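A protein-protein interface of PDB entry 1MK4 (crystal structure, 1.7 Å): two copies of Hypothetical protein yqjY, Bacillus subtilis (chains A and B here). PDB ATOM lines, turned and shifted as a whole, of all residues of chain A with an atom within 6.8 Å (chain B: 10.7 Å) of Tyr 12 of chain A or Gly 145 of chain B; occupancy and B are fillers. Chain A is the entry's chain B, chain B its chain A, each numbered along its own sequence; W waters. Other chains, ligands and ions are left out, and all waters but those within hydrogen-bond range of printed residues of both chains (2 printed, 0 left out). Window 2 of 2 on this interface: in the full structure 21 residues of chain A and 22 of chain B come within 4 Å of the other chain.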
ATOM      1  N   THR A   8      15.297 -35.825   0.491  1.00  0.00           N
ATOM      2  CA  THR A   8      13.931 -35.535   0.884  1.00  0.00           C
ATOM      3  C   THR A   8      13.729 -34.050   0.593  1.00  0.00           C
ATOM      4  O   THR A   8      14.699 -33.325   0.374  1.00  0.00           O
ATOM      5  CB  THR A   8      13.699 -35.825   2.381  1.00  0.00           C
ATOM      6  OG1 THR A   8      12.300 -35.717   2.673  1.00  0.00           O
ATOM      7  CG2 THR A   8      14.470 -34.844   3.241  1.00  0.00           C
ATOM      8  N   SER A   9      12.484 -33.593   0.581  1.00  0.00           N
ATOM      9  CA  SER A   9      12.222 -32.192   0.283  1.00  0.00           C
ATOM     10  C   SER A   9      12.951 -31.248   1.235  1.00  0.00           C
ATOM     11  O   SER A   9      13.407 -30.179   0.824  1.00  0.00           O
ATOM     12  CB  SER A   9      10.718 -31.908   0.328  1.00  0.00           C
ATOM     13  OG  SER A   9      10.431 -30.676  -0.317  1.00  0.00           O
ATOM     14  N   SER A  10      13.078 -31.650   2.496  1.00  0.00           N
ATOM     15  CA  SER A  10      13.739 -30.817   3.498  1.00  0.00           C
ATOM     16  C   SER A  10      15.248 -30.647   3.311  1.00  0.00           C
ATOM     17  O   SER A  10      15.863 -29.822   3.985  1.00  0.00           O
ATOM     18  CB  SER A  10      13.451 -31.350   4.905  1.00  0.00           C
ATOM     19  OG  SER A  10      13.969 -32.654   5.083  1.00  0.00           O
ATOM     20  N   ASP A  11      15.847 -31.413   2.404  1.00  0.00           N
ATOM     21  CA  ASP A  11      17.283 -31.290   2.151  1.00  0.00           C
ATOM     22  C   ASP A  11      17.577 -30.098   1.250  1.00  0.00           C
ATOM     23  O   ASP A  11      18.736 -29.732   1.053  1.00  0.00           O
ATOM     24  CB  ASP A  11      17.839 -32.549   1.474  1.00  0.00           C
ATOM     25  CG  ASP A  11      17.855 -33.753   2.388  1.00  0.00           C
ATOM     26  OD1 ASP A  11      18.312 -33.620   3.546  1.00  0.00           O
ATOM     27  OD2 ASP A  11      17.423 -34.840   1.946  1.00  0.00           O
ATOM     28  N   TYR A  12      16.531 -29.489   0.699  1.00  0.00           N
ATOM     29  CA  TYR A  12      16.706 -28.362  -0.212  1.00  0.00           C
ATOM     30  C   TYR A  12      17.628 -27.244   0.281  1.00  0.00           C
ATOM     31  O   TYR A  12      18.574 -26.859  -0.411  1.00  0.00           O
ATOM     32  CB  TYR A  12      15.349 -27.755  -0.572  1.00  0.00           C
ATOM     33  CG  TYR A  12      15.464 -26.582  -1.518  1.00  0.00           C
ATOM     34  CD1 TYR A  12      15.793 -26.773  -2.860  1.00  0.00           C
ATOM     35  CD2 TYR A  12      15.284 -25.279  -1.062  1.00  0.00           C
ATOM     36  CE1 TYR A  12      15.939 -25.688  -3.726  1.00  0.00           C
ATOM     37  CE2 TYR A  12      15.430 -24.192  -1.915  1.00  0.00           C
ATOM     38  CZ  TYR A  12      15.757 -24.400  -3.242  1.00  0.00           C
ATOM     39  OH  TYR A  12      15.899 -23.317  -4.079  1.00  0.00           O
ATOM     40  N   GLU A  13      17.348 -26.719   1.468  1.00  0.00           N
ATOM     41  CA  GLU A  13      18.146 -25.629   2.021  1.00  0.00           C
ATOM     42  C   GLU A  13      19.604 -26.027   2.237  1.00  0.00           C
ATOM     43  O   GLU A  13      20.520 -25.317   1.817  1.00  0.00           O
ATOM     44  CB  GLU A  13      17.543 -25.154   3.348  1.00  0.00           C
ATOM     45  CG  GLU A  13      18.029 -23.778   3.775  1.00  0.00           C
ATOM     46  CD  GLU A  13      17.643 -23.424   5.199  1.00  0.00           C
ATOM     47  OE1 GLU A  13      16.482 -23.670   5.591  1.00  0.00           O
ATOM     48  OE2 GLU A  13      18.504 -22.883   5.925  1.00  0.00           O
ATOM     49  N   MET A  14      19.813 -27.162   2.893  1.00  0.00           N
ATOM     50  CA  MET A  14      21.160 -27.648   3.173  1.00  0.00           C
ATOM     51  C   MET A  14      21.983 -27.833   1.895  1.00  0.00           C
ATOM     52  O   MET A  14      23.087 -27.299   1.781  1.00  0.00           O
ATOM     53  CB  MET A  14      21.081 -28.966   3.958  1.00  0.00           C
ATOM     54  CG  MET A  14      22.416 -29.491   4.490  1.00  0.00           C
ATOM     55  SD  MET A  14      23.378 -30.407   3.278  1.00  0.00           S
ATOM     56  CE  MET A  14      22.699 -32.056   3.526  1.00  0.00           C
ATOM     57  N   VAL A  15      21.443 -28.566   0.926  1.00  0.00           N
ATOM     58  CA  VAL A  15      22.160 -28.816  -0.323  1.00  0.00           C
ATOM     59  C   VAL A  15      22.478 -27.574  -1.159  1.00  0.00           C
ATOM     60  O   VAL A  15      23.600 -27.419  -1.642  1.00  0.00           O
ATOM     61  CB  VAL A  15      21.391 -29.824  -1.211  1.00  0.00           C
ATOM     62  CG1 VAL A  15      22.115 -30.018  -2.535  1.00  0.00           C
ATOM     63  CG2 VAL A  15      21.262 -31.157  -0.484  1.00  0.00           C
ATOM     64  N   THR A  16      21.502 -26.688  -1.338  1.00  0.00           N
ATOM     65  CA  THR A  16      21.730 -25.488  -2.139  1.00  0.00           C
ATOM     66  C   THR A  16      22.693 -24.495  -1.487  1.00  0.00           C
ATOM     67  O   THR A  16      23.441 -23.809  -2.178  1.00  0.00           O
ATOM     68  CB  THR A  16      20.404 -24.761  -2.459  1.00  0.00           C
ATOM     69  OG1 THR A  16      19.713 -24.462  -1.244  1.00  0.00           O
ATOM     70  CG2 THR A  16      19.520 -25.630  -3.342  1.00  0.00           C
ATOM     71  N   SER A  17      22.685 -24.417  -0.162  1.00  0.00           N
ATOM     72  CA  SER A  17      23.578 -23.491   0.525  1.00  0.00           C
ATOM     73  C   SER A  17      25.010 -24.017   0.547  1.00  0.00           C
ATOM     74  O   SER A  17      25.958 -23.269   0.305  1.00  0.00           O
ATOM     75  CB  SER A  17      23.092 -23.242   1.952  1.00  0.00           C
ATOM     76  OG  SER A  17      23.047 -24.448   2.690  1.00  0.00           O
ATOM     77  N   GLU A  30      20.906 -20.131 -11.150  1.00  0.00           N
ATOM     78  CA  GLU A  30      20.136 -21.164 -10.462  1.00  0.00           C
ATOM     79  C   GLU A  30      19.838 -22.315 -11.406  1.00  0.00           C
ATOM     80  O   GLU A  30      19.247 -22.119 -12.470  1.00  0.00           O
ATOM     81  CB  GLU A  30      18.816 -20.598  -9.935  1.00  0.00           C
ATOM     82  CG  GLU A  30      18.958 -19.578  -8.818  1.00  0.00           C
ATOM     83  CD  GLU A  30      17.611 -19.157  -8.258  1.00  0.00           C
ATOM     84  OE1 GLU A  30      16.787 -18.611  -9.029  1.00  0.00           O
ATOM     85  OE2 GLU A  30      17.372 -19.374  -7.050  1.00  0.00           O
ATOM     86  N   LEU A  32      19.072 -25.578  -9.771  1.00  0.00           N
ATOM     87  CA  LEU A  32      18.435 -26.590  -8.930  1.00  0.00           C
ATOM     88  C   LEU A  32      17.140 -26.157  -8.253  1.00  0.00           C
ATOM     89  O   LEU A  32      17.102 -25.948  -7.040  1.00  0.00           O
ATOM     90  CB  LEU A  32      19.402 -27.080  -7.850  1.00  0.00           C
ATOM     91  CG  LEU A  32      20.515 -28.041  -8.262  1.00  0.00           C
ATOM     92  CD1 LEU A  32      21.320 -28.410  -7.030  1.00  0.00           C
ATOM     93  CD2 LEU A  32      19.920 -29.291  -8.900  1.00  0.00           C
ATOM     94  N   PRO A  33      16.056 -26.010  -9.028  1.00  0.00           N
ATOM     95  CA  PRO A  33      14.789 -25.604  -8.417  1.00  0.00           C
ATOM     96  C   PRO A  33      14.273 -26.703  -7.486  1.00  0.00           C
ATOM     97  O   PRO A  33      14.647 -27.874  -7.612  1.00  0.00           O
ATOM     98  CB  PRO A  33      13.883 -25.364  -9.623  1.00  0.00           C
ATOM     99  CG  PRO A  33      14.444 -26.303 -10.661  1.00  0.00           C
ATOM    100  CD  PRO A  33      15.927 -26.114 -10.492  1.00  0.00           C
ATOM    101  N   ARG A  34      13.419 -26.308  -6.549  1.00  0.00           N
ATOM    102  CA  ARG A  34      12.842 -27.209  -5.558  1.00  0.00           C
ATOM    103  C   ARG A  34      12.187 -28.468  -6.133  1.00  0.00           C
ATOM    104  O   ARG A  34      12.239 -29.530  -5.514  1.00  0.00           O
ATOM    105  CB  ARG A  34      11.827 -26.432  -4.705  1.00  0.00           C
ATOM    106  CG  ARG A  34      11.261 -27.176  -3.500  1.00  0.00           C
ATOM    107  CD  ARG A  34      12.347 -27.551  -2.512  1.00  0.00           C
ATOM    108  NE  ARG A  34      11.814 -28.067  -1.252  1.00  0.00           N
ATOM    109  CZ  ARG A  34      11.584 -27.326  -0.171  1.00  0.00           C
ATOM    110  NH1 ARG A  34      11.835 -26.025  -0.182  1.00  0.00           N
ATOM    111  NH2 ARG A  34      11.116 -27.891   0.932  1.00  0.00           N
ATOM    112  N   LEU A  35      11.583 -28.356  -7.313  1.00  0.00           N
ATOM    113  CA  LEU A  35      10.909 -29.504  -7.924  1.00  0.00           C
ATOM    114  C   LEU A  35      11.769 -30.774  -7.978  1.00  0.00           C
ATOM    115  O   LEU A  35      11.249 -31.883  -7.879  1.00  0.00           O
ATOM    116  CB  LEU A  35      10.420 -29.139  -9.332  1.00  0.00           C
ATOM    117  CG  LEU A  35      11.463 -28.894 -10.424  1.00  0.00           C
ATOM    118  CD1 LEU A  35      11.818 -30.213 -11.094  1.00  0.00           C
ATOM    119  CD2 LEU A  35      10.904 -27.914 -11.450  1.00  0.00           C
ATOM    120  N   PHE A  37      13.940 -31.835  -5.754  1.00  0.00           N
ATOM    121  CA  PHE A  37      13.968 -32.448  -4.423  1.00  0.00           C
ATOM    122  C   PHE A  37      12.631 -33.045  -4.016  1.00  0.00           C
ATOM    123  O   PHE A  37      12.548 -33.833  -3.073  1.00  0.00           O
ATOM    124  CB  PHE A  37      14.373 -31.414  -3.367  1.00  0.00           C
ATOM    125  CG  PHE A  37      15.763 -30.885  -3.538  1.00  0.00           C
ATOM    126  CD1 PHE A  37      16.068 -30.008  -4.574  1.00  0.00           C
ATOM    127  CD2 PHE A  37      16.780 -31.287  -2.675  1.00  0.00           C
ATOM    128  CE1 PHE A  37      17.365 -29.540  -4.752  1.00  0.00           C
ATOM    129  CE2 PHE A  37      18.081 -30.825  -2.846  1.00  0.00           C
ATOM    130  CZ  PHE A  37      18.376 -29.952  -3.884  1.00  0.00           C
ATOM    131  N   ILE A  46      22.411 -38.287  -1.200  1.00  0.00           N
ATOM    132  CA  ILE A  46      23.304 -37.455  -0.410  1.00  0.00           C
ATOM    133  C   ILE A  46      24.237 -38.397   0.348  1.00  0.00           C
ATOM    134  O   ILE A  46      23.784 -39.357   0.968  1.00  0.00           O
ATOM    135  CB  ILE A  46      22.528 -36.594   0.611  1.00  0.00           C
ATOM    136  CG1 ILE A  46      21.807 -35.449  -0.112  1.00  0.00           C
ATOM    137  CG2 ILE A  46      23.490 -36.029   1.663  1.00  0.00           C
ATOM    138  CD1 ILE A  46      20.849 -34.679   0.778  1.00  0.00           C
ATOM    139  N   LYS B  29      13.111 -14.570 -15.161  1.00  0.00           N
ATOM    140  CA  LYS B  29      14.243 -15.139 -14.446  1.00  0.00           C
ATOM    141  C   LYS B  29      14.315 -16.620 -14.782  1.00  0.00           C
ATOM    142  O   LYS B  29      15.347 -17.117 -15.235  1.00  0.00           O
ATOM    143  CB  LYS B  29      14.067 -14.949 -12.934  1.00  0.00           C
ATOM    144  CG  LYS B  29      14.989 -15.807 -12.066  1.00  0.00           C
ATOM    145  CD  LYS B  29      16.464 -15.567 -12.370  1.00  0.00           C
ATOM    146  CE  LYS B  29      17.345 -16.508 -11.555  1.00  0.00           C
ATOM    147  NZ  LYS B  29      18.799 -16.321 -11.852  1.00  0.00           N
ATOM    148  N   GLU B  30      13.202 -17.317 -14.576  1.00  0.00           N
ATOM    149  CA  GLU B  30      13.137 -18.744 -14.849  1.00  0.00           C
ATOM    150  C   GLU B  30      13.390 -19.064 -16.317  1.00  0.00           C
ATOM    151  O   GLU B  30      12.818 -18.440 -17.217  1.00  0.00           O
ATOM    152  CB  GLU B  30      11.775 -19.303 -14.425  1.00  0.00           C
ATOM    153  CG  GLU B  30      11.481 -19.171 -12.933  1.00  0.00           C
ATOM    154  CD  GLU B  30      12.438 -19.975 -12.065  1.00  0.00           C
ATOM    155  OE1 GLU B  30      13.655 -19.680 -12.078  1.00  0.00           O
ATOM    156  OE2 GLU B  30      11.970 -20.903 -11.368  1.00  0.00           O
ATOM    157  N   VAL B 108       3.199 -24.539  -8.997  1.00  0.00           N
ATOM    158  CA  VAL B 108       3.439 -23.462  -8.047  1.00  0.00           C
ATOM    159  C   VAL B 108       3.530 -22.100  -8.704  1.00  0.00           C
ATOM    160  O   VAL B 108       3.638 -21.982  -9.927  1.00  0.00           O
ATOM    161  CB  VAL B 108       4.769 -23.685  -7.268  1.00  0.00           C
ATOM    162  CG1 VAL B 108       4.781 -25.057  -6.618  1.00  0.00           C
ATOM    163  CG2 VAL B 108       5.959 -23.538  -8.216  1.00  0.00           C
ATOM    164  N   SER B 110       4.253 -17.550  -7.451  1.00  0.00           N
ATOM    165  CA  SER B 110       4.611 -16.606  -6.403  1.00  0.00           C
ATOM    166  C   SER B 110       3.341 -16.041  -5.789  1.00  0.00           C
ATOM    167  O   SER B 110       2.327 -15.911  -6.470  1.00  0.00           O
ATOM    168  CB  SER B 110       5.434 -15.460  -6.988  1.00  0.00           C
ATOM    169  OG  SER B 110       5.498 -14.381  -6.072  1.00  0.00           O
ATOM    170  N   PRO B 111       3.380 -15.699  -4.490  1.00  0.00           N
ATOM    171  CA  PRO B 111       2.220 -15.140  -3.791  1.00  0.00           C
ATOM    172  C   PRO B 111       1.728 -13.820  -4.399  1.00  0.00           C
ATOM    173  O   PRO B 111       0.569 -13.446  -4.225  1.00  0.00           O
ATOM    174  CB  PRO B 111       2.736 -14.946  -2.364  1.00  0.00           C
ATOM    175  CG  PRO B 111       3.771 -16.014  -2.224  1.00  0.00           C
ATOM    176  CD  PRO B 111       4.484 -15.960  -3.550  1.00  0.00           C
ATOM    177  N   LYS B 132       3.025 -19.922   6.297  1.00  0.00           N
ATOM    178  CA  LYS B 132       2.725 -18.508   6.465  1.00  0.00           C
ATOM    179  C   LYS B 132       1.568 -18.123   5.560  1.00  0.00           C
ATOM    180  O   LYS B 132       1.104 -18.924   4.749  1.00  0.00           O
ATOM    181  CB  LYS B 132       3.957 -17.647   6.146  1.00  0.00           C
ATOM    182  CG  LYS B 132       4.521 -17.838   4.752  1.00  0.00           C
ATOM    183  CD  LYS B 132       5.824 -17.059   4.542  1.00  0.00           C
ATOM    184  CE  LYS B 132       5.596 -15.568   4.383  1.00  0.00           C
ATOM    185  NZ  LYS B 132       6.866 -14.849   4.043  1.00  0.00           N
ATOM    186  N   VAL B 139       1.011 -19.913   2.084  1.00  0.00           N
ATOM    187  CA  VAL B 139       2.272 -19.950   1.358  1.00  0.00           C
ATOM    188  C   VAL B 139       3.362 -20.784   2.024  1.00  0.00           C
ATOM    189  O   VAL B 139       3.406 -20.918   3.247  1.00  0.00           O
ATOM    190  CB  VAL B 139       2.797 -18.500   1.175  1.00  0.00           C
ATOM    191  CG1 VAL B 139       4.223 -18.497   0.651  1.00  0.00           C
ATOM    192  CG2 VAL B 139       1.881 -17.745   0.223  1.00  0.00           C
ATOM    193  N   PHE B 140       4.238 -21.352   1.201  1.00  0.00           N
ATOM    194  CA  PHE B 140       5.365 -22.128   1.703  1.00  0.00           C
ATOM    195  C   PHE B 140       6.562 -21.182   1.697  1.00  0.00           C
ATOM    196  O   PHE B 140       7.069 -20.808   0.642  1.00  0.00           O
ATOM    197  CB  PHE B 140       5.623 -23.348   0.810  1.00  0.00           C
ATOM    198  CG  PHE B 140       4.674 -24.492   1.065  1.00  0.00           C
ATOM    199  CD1 PHE B 140       3.318 -24.376   0.765  1.00  0.00           C
ATOM    200  CD2 PHE B 140       5.135 -25.675   1.640  1.00  0.00           C
ATOM    201  CE1 PHE B 140       2.437 -25.422   1.034  1.00  0.00           C
ATOM    202  CE2 PHE B 140       4.261 -26.731   1.916  1.00  0.00           C
ATOM    203  CZ  PHE B 140       2.908 -26.605   1.613  1.00  0.00           C
ATOM    204  N   ALA B 141       6.992 -20.777   2.887  1.00  0.00           N
ATOM    205  CA  ALA B 141       8.106 -19.847   3.026  1.00  0.00           C
ATOM    206  C   ALA B 141       9.410 -20.335   2.407  1.00  0.00           C
ATOM    207  O   ALA B 141       9.833 -21.470   2.635  1.00  0.00           O
ATOM    208  CB  ALA B 141       8.327 -19.524   4.503  1.00  0.00           C
ATOM    209  N   ASN B 142      10.029 -19.458   1.619  1.00  0.00           N
ATOM    210  CA  ASN B 142      11.310 -19.726   0.964  1.00  0.00           C
ATOM    211  C   ASN B 142      11.373 -21.078   0.261  1.00  0.00           C
ATOM    212  O   ASN B 142      12.414 -21.736   0.259  1.00  0.00           O
ATOM    213  CB  ASN B 142      12.438 -19.633   1.997  1.00  0.00           C
ATOM    214  CG  ASN B 142      12.374 -18.353   2.814  1.00  0.00           C
ATOM    215  OD1 ASN B 142      12.459 -17.251   2.273  1.00  0.00           O
ATOM    216  ND2 ASN B 142      12.217 -18.496   4.123  1.00  0.00           N
ATOM    217  N   TYR B 143      10.261 -21.476  -0.346  1.00  0.00           N
ATOM    218  CA  TYR B 143      10.169 -22.752  -1.046  1.00  0.00           C
ATOM    219  C   TYR B 143      11.252 -22.939  -2.108  1.00  0.00           C
ATOM    220  O   TYR B 143      11.863 -24.010  -2.200  1.00  0.00           O
ATOM    221  CB  TYR B 143       8.792 -22.885  -1.701  1.00  0.00           C
ATOM    222  CG  TYR B 143       8.459 -24.296  -2.120  1.00  0.00           C
ATOM    223  CD1 TYR B 143       8.265 -25.295  -1.167  1.00  0.00           C
ATOM    224  CD2 TYR B 143       8.341 -24.637  -3.467  1.00  0.00           C
ATOM    225  CE1 TYR B 143       7.962 -26.602  -1.542  1.00  0.00           C
ATOM    226  CE2 TYR B 143       8.036 -25.945  -3.853  1.00  0.00           C
ATOM    227  CZ  TYR B 143       7.850 -26.919  -2.886  1.00  0.00           C
ATOM    228  OH  TYR B 143       7.569 -28.217  -3.252  1.00  0.00           O
ATOM    229  N   ASP B 144      11.480 -21.905  -2.915  1.00  0.00           N
ATOM    230  CA  ASP B 144      12.496 -21.961  -3.966  1.00  0.00           C
ATOM    231  C   ASP B 144      13.752 -21.168  -3.600  1.00  0.00           C
ATOM    232  O   ASP B 144      14.451 -20.668  -4.481  1.00  0.00           O
ATOM    233  CB  ASP B 144      11.940 -21.426  -5.293  1.00  0.00           C
ATOM    234  CG  ASP B 144      11.269 -22.503  -6.129  1.00  0.00           C
ATOM    235  OD1 ASP B 144      11.884 -23.569  -6.324  1.00  0.00           O
ATOM    236  OD2 ASP B 144      10.134 -22.280  -6.605  1.00  0.00           O
ATOM    237  N   GLY B 145      14.030 -21.056  -2.305  1.00  0.00           N
ATOM    238  CA  GLY B 145      15.206 -20.320  -1.864  1.00  0.00           C
ATOM    239  C   GLY B 145      14.849 -19.128  -0.994  1.00  0.00           C
ATOM    240  O   GLY B 145      13.673 -18.809  -0.839  1.00  0.00           O
ATOM    241  N   PRO B 146      15.844 -18.443  -0.410  1.00  0.00           N
ATOM    242  CA  PRO B 146      15.557 -17.285   0.442  1.00  0.00           C
ATOM    243  C   PRO B 146      14.770 -16.190  -0.268  1.00  0.00           C
ATOM    244  O   PRO B 146      15.124 -15.763  -1.367  1.00  0.00           O
ATOM    245  CB  PRO B 146      16.949 -16.826   0.893  1.00  0.00           C
ATOM    246  CG  PRO B 146      17.845 -17.305  -0.203  1.00  0.00           C
ATOM    247  CD  PRO B 146      17.294 -18.673  -0.513  1.00  0.00           C
ATOM    248  N   GLY B 147      13.686 -15.754   0.364  1.00  0.00           N
ATOM    249  CA  GLY B 147      12.856 -14.720  -0.219  1.00  0.00           C
ATOM    250  C   GLY B 147      12.033 -15.212  -1.396  1.00  0.00           C
ATOM    251  O   GLY B 147      11.406 -14.411  -2.094  1.00  0.00           O
ATOM    252  N   GLN B 148      12.030 -16.523  -1.627  1.00  0.00           N
ATOM    253  CA  GLN B 148      11.265 -17.086  -2.736  1.00  0.00           C
ATOM    254  C   GLN B 148      10.071 -17.898  -2.242  1.00  0.00           C
ATOM    255  O   GLN B 148      10.027 -19.119  -2.408  1.00  0.00           O
ATOM    256  CB  GLN B 148      12.155 -17.972  -3.615  1.00  0.00           C
ATOM    257  CG  GLN B 148      13.281 -17.241  -4.341  1.00  0.00           C
ATOM    258  CD  GLN B 148      12.778 -16.123  -5.244  1.00  0.00           C
ATOM    259  OE1 GLN B 148      11.886 -16.325  -6.071  1.00  0.00           O
ATOM    260  NE2 GLN B 148      13.361 -14.937  -5.096  1.00  0.00           N
ATOM    261  N   ASP B 149       9.107 -17.218  -1.630  1.00  0.00           N
ATOM    262  CA  ASP B 149       7.913 -17.890  -1.134  1.00  0.00           C
ATOM    263  C   ASP B 149       7.117 -18.403  -2.324  1.00  0.00           C
ATOM    264  O   ASP B 149       7.159 -17.824  -3.411  1.00  0.00           O
ATOM    265  CB  ASP B 149       7.031 -16.932  -0.327  1.00  0.00           C
ATOM    266  CG  ASP B 149       7.754 -16.319   0.857  1.00  0.00           C
ATOM    267  OD1 ASP B 149       8.676 -16.964   1.407  1.00  0.00           O
ATOM    268  OD2 ASP B 149       7.377 -15.191   1.248  1.00  0.00           O
ATOM    269  N   ARG B 150       6.385 -19.487  -2.120  1.00  0.00           N
ATOM    270  CA  ARG B 150       5.596 -20.051  -3.201  1.00  0.00           C
ATOM    271  C   ARG B 150       4.227 -20.520  -2.747  1.00  0.00           C
ATOM    272  O   ARG B 150       4.051 -20.975  -1.615  1.00  0.00           O
ATOM    273  CB  ARG B 150       6.331 -21.243  -3.828  1.00  0.00           C
ATOM    274  CG  ARG B 150       7.618 -20.888  -4.562  1.00  0.00           C
ATOM    275  CD  ARG B 150       7.340 -20.134  -5.858  1.00  0.00           C
ATOM    276  NE  ARG B 150       8.571 -19.781  -6.560  1.00  0.00           N
ATOM    277  CZ  ARG B 150       9.265 -18.667  -6.341  1.00  0.00           C
ATOM    278  NH1 ARG B 150       8.849 -17.787  -5.440  1.00  0.00           N
ATOM    279  NH2 ARG B 150      10.376 -18.430  -7.025  1.00  0.00           N
ATOM    280  N   LEU B 152       1.520 -23.272  -3.407  1.00  0.00           N
ATOM    281  CA  LEU B 152       1.480 -24.614  -3.983  1.00  0.00           C
ATOM    282  C   LEU B 152       0.044 -25.017  -4.318  1.00  0.00           C
ATOM    283  O   LEU B 152      -0.812 -25.091  -3.429  1.00  0.00           O
ATOM    284  CB  LEU B 152       2.092 -25.629  -3.004  1.00  0.00           C
ATOM    285  CG  LEU B 152       3.616 -25.818  -3.077  1.00  0.00           C
ATOM    286  CD1 LEU B 152       4.322 -24.479  -2.878  1.00  0.00           C
ATOM    287  CD2 LEU B 152       4.063 -26.825  -2.020  1.00  0.00           C
HETATM  288  O   HOH W   1      10.692 -25.469  -8.073  1.00  0.00           O
HETATM  289  O   HOH W   2       7.999 -30.229  -1.121  1.00  0.00           O
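Water W2 bridges OG of Ser 9 of chain A (2.6 Å) and OH of Tyr 143 of chain B (3.0 Å). Water W1 lies within hydrogen-bond range of the side-chain carboxylate (OD1) of Asp 144 of chain B, the backbone NH (N) of Leu 35 of chain A and the backbone NH (N) of Arg 34 of chain A.
NH1 of Arg 34 of chain A lies within hydrogen-bond range of O of Tyr 143 of chain B (2.9 Å). The backbone carbonyl oxygen of Asp 144 of chain B lies within hydrogen-bond range of the side-chain hydroxyl of Tyr 12 of chain A (3.0 Å). The side-chain carboxylate (OD1) of Asp 144 of chain B lies within hydrogen-bond range of the backbone NH (N) of Arg 34 of chain A (3.1 Å). The side-chain hydroxyl of Tyr 12 of chain A lies within hydrogen-bond range of the backbone NH of Gly 145 of chain B, 3.4 Å away.
Among the printed residues, pairs that only touch across the chains: Tyr 12 of chain A with Tyr 143 of chain B and Glu 30 of chain A with Lys 29 of chain B.
No residue of chain B comes within 4 Å of Ser 9 of chain A. No residue of chain B comes within 4 Å of Ser 10 of chain A. No residue of chain B comes within 4 Å of Asp 11 of chain A. No residue of chain B comes within 4 Å of Val 15 of chain A. No residue of chain B comes within 4 Å of Thr 16 of chain A. Of the printed residues of chain B, Glu 30 of chain A touches Lys 29 (3.3 Å). Of chain B, only Tyr 143 and Asp 144 come within 4 Å of Arg 34 of chain A. Printed residues of chain A within 4 Å of Lys 29 of chain B: Glu 30 (3.3 Å). Of the printed residues of chain A, Tyr 143 of chain B touches Tyr 12 (3.6 Å) and Arg 34 (2.9 Å). Printed residues of chain A within 4 Å of Asp 144 of chain B: Tyr 12 (3.0 Å) and Arg 34 (3.1 Å). Of the printed residues of chain A, Gly 145 of chain B touches Tyr 12. Gly 147 of chain B touches none of the printed residues of chain A. Asp 149 of chain B touches none of the printed residues of chain A. The nearest residue of chain A that does not touch Gly 145 of chain B is Glu 30 of chain A (5.7 Å).
N of Tyr 143 of chain B lies within hydrogen-bond range of O of Gln 148 of chain B, 3.1 Å away. The side-chain carboxylate (OD2) of Asp 144 of chain B is in salt-bridge range of the guanidinium group (NE) of Arg 150 of chain B. NE of Arg 34 of chain A sits at hydrogen-bond distance from OG of Ser 9 of chain A, at 3.1 Å. O of Tyr 12 of chain A lies within hydrogen-bond range of OG1 of Thr 16 of chain A, 2.8 Å away.
1 position is printed for both chains.
Of the 19 printed residues of chain B, 4 touch a printed residue of chain A. Hydrophobic or aromatic side chains of chain B that line the printed part of chain A: Tyr 143. Of the 17 printed residues of chain A, 3 touch a printed residue of chain B. Hydrophobic or aromatic side chains of chain A that line the printed part of chain B: Tyr 12. Among the printed residues, 6 pairs touch across the chains. Among the printed residues, no Asp or Glu carboxylate lies within 4 Å of a Lys or Arg side-chain nitrogen of the other chain.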
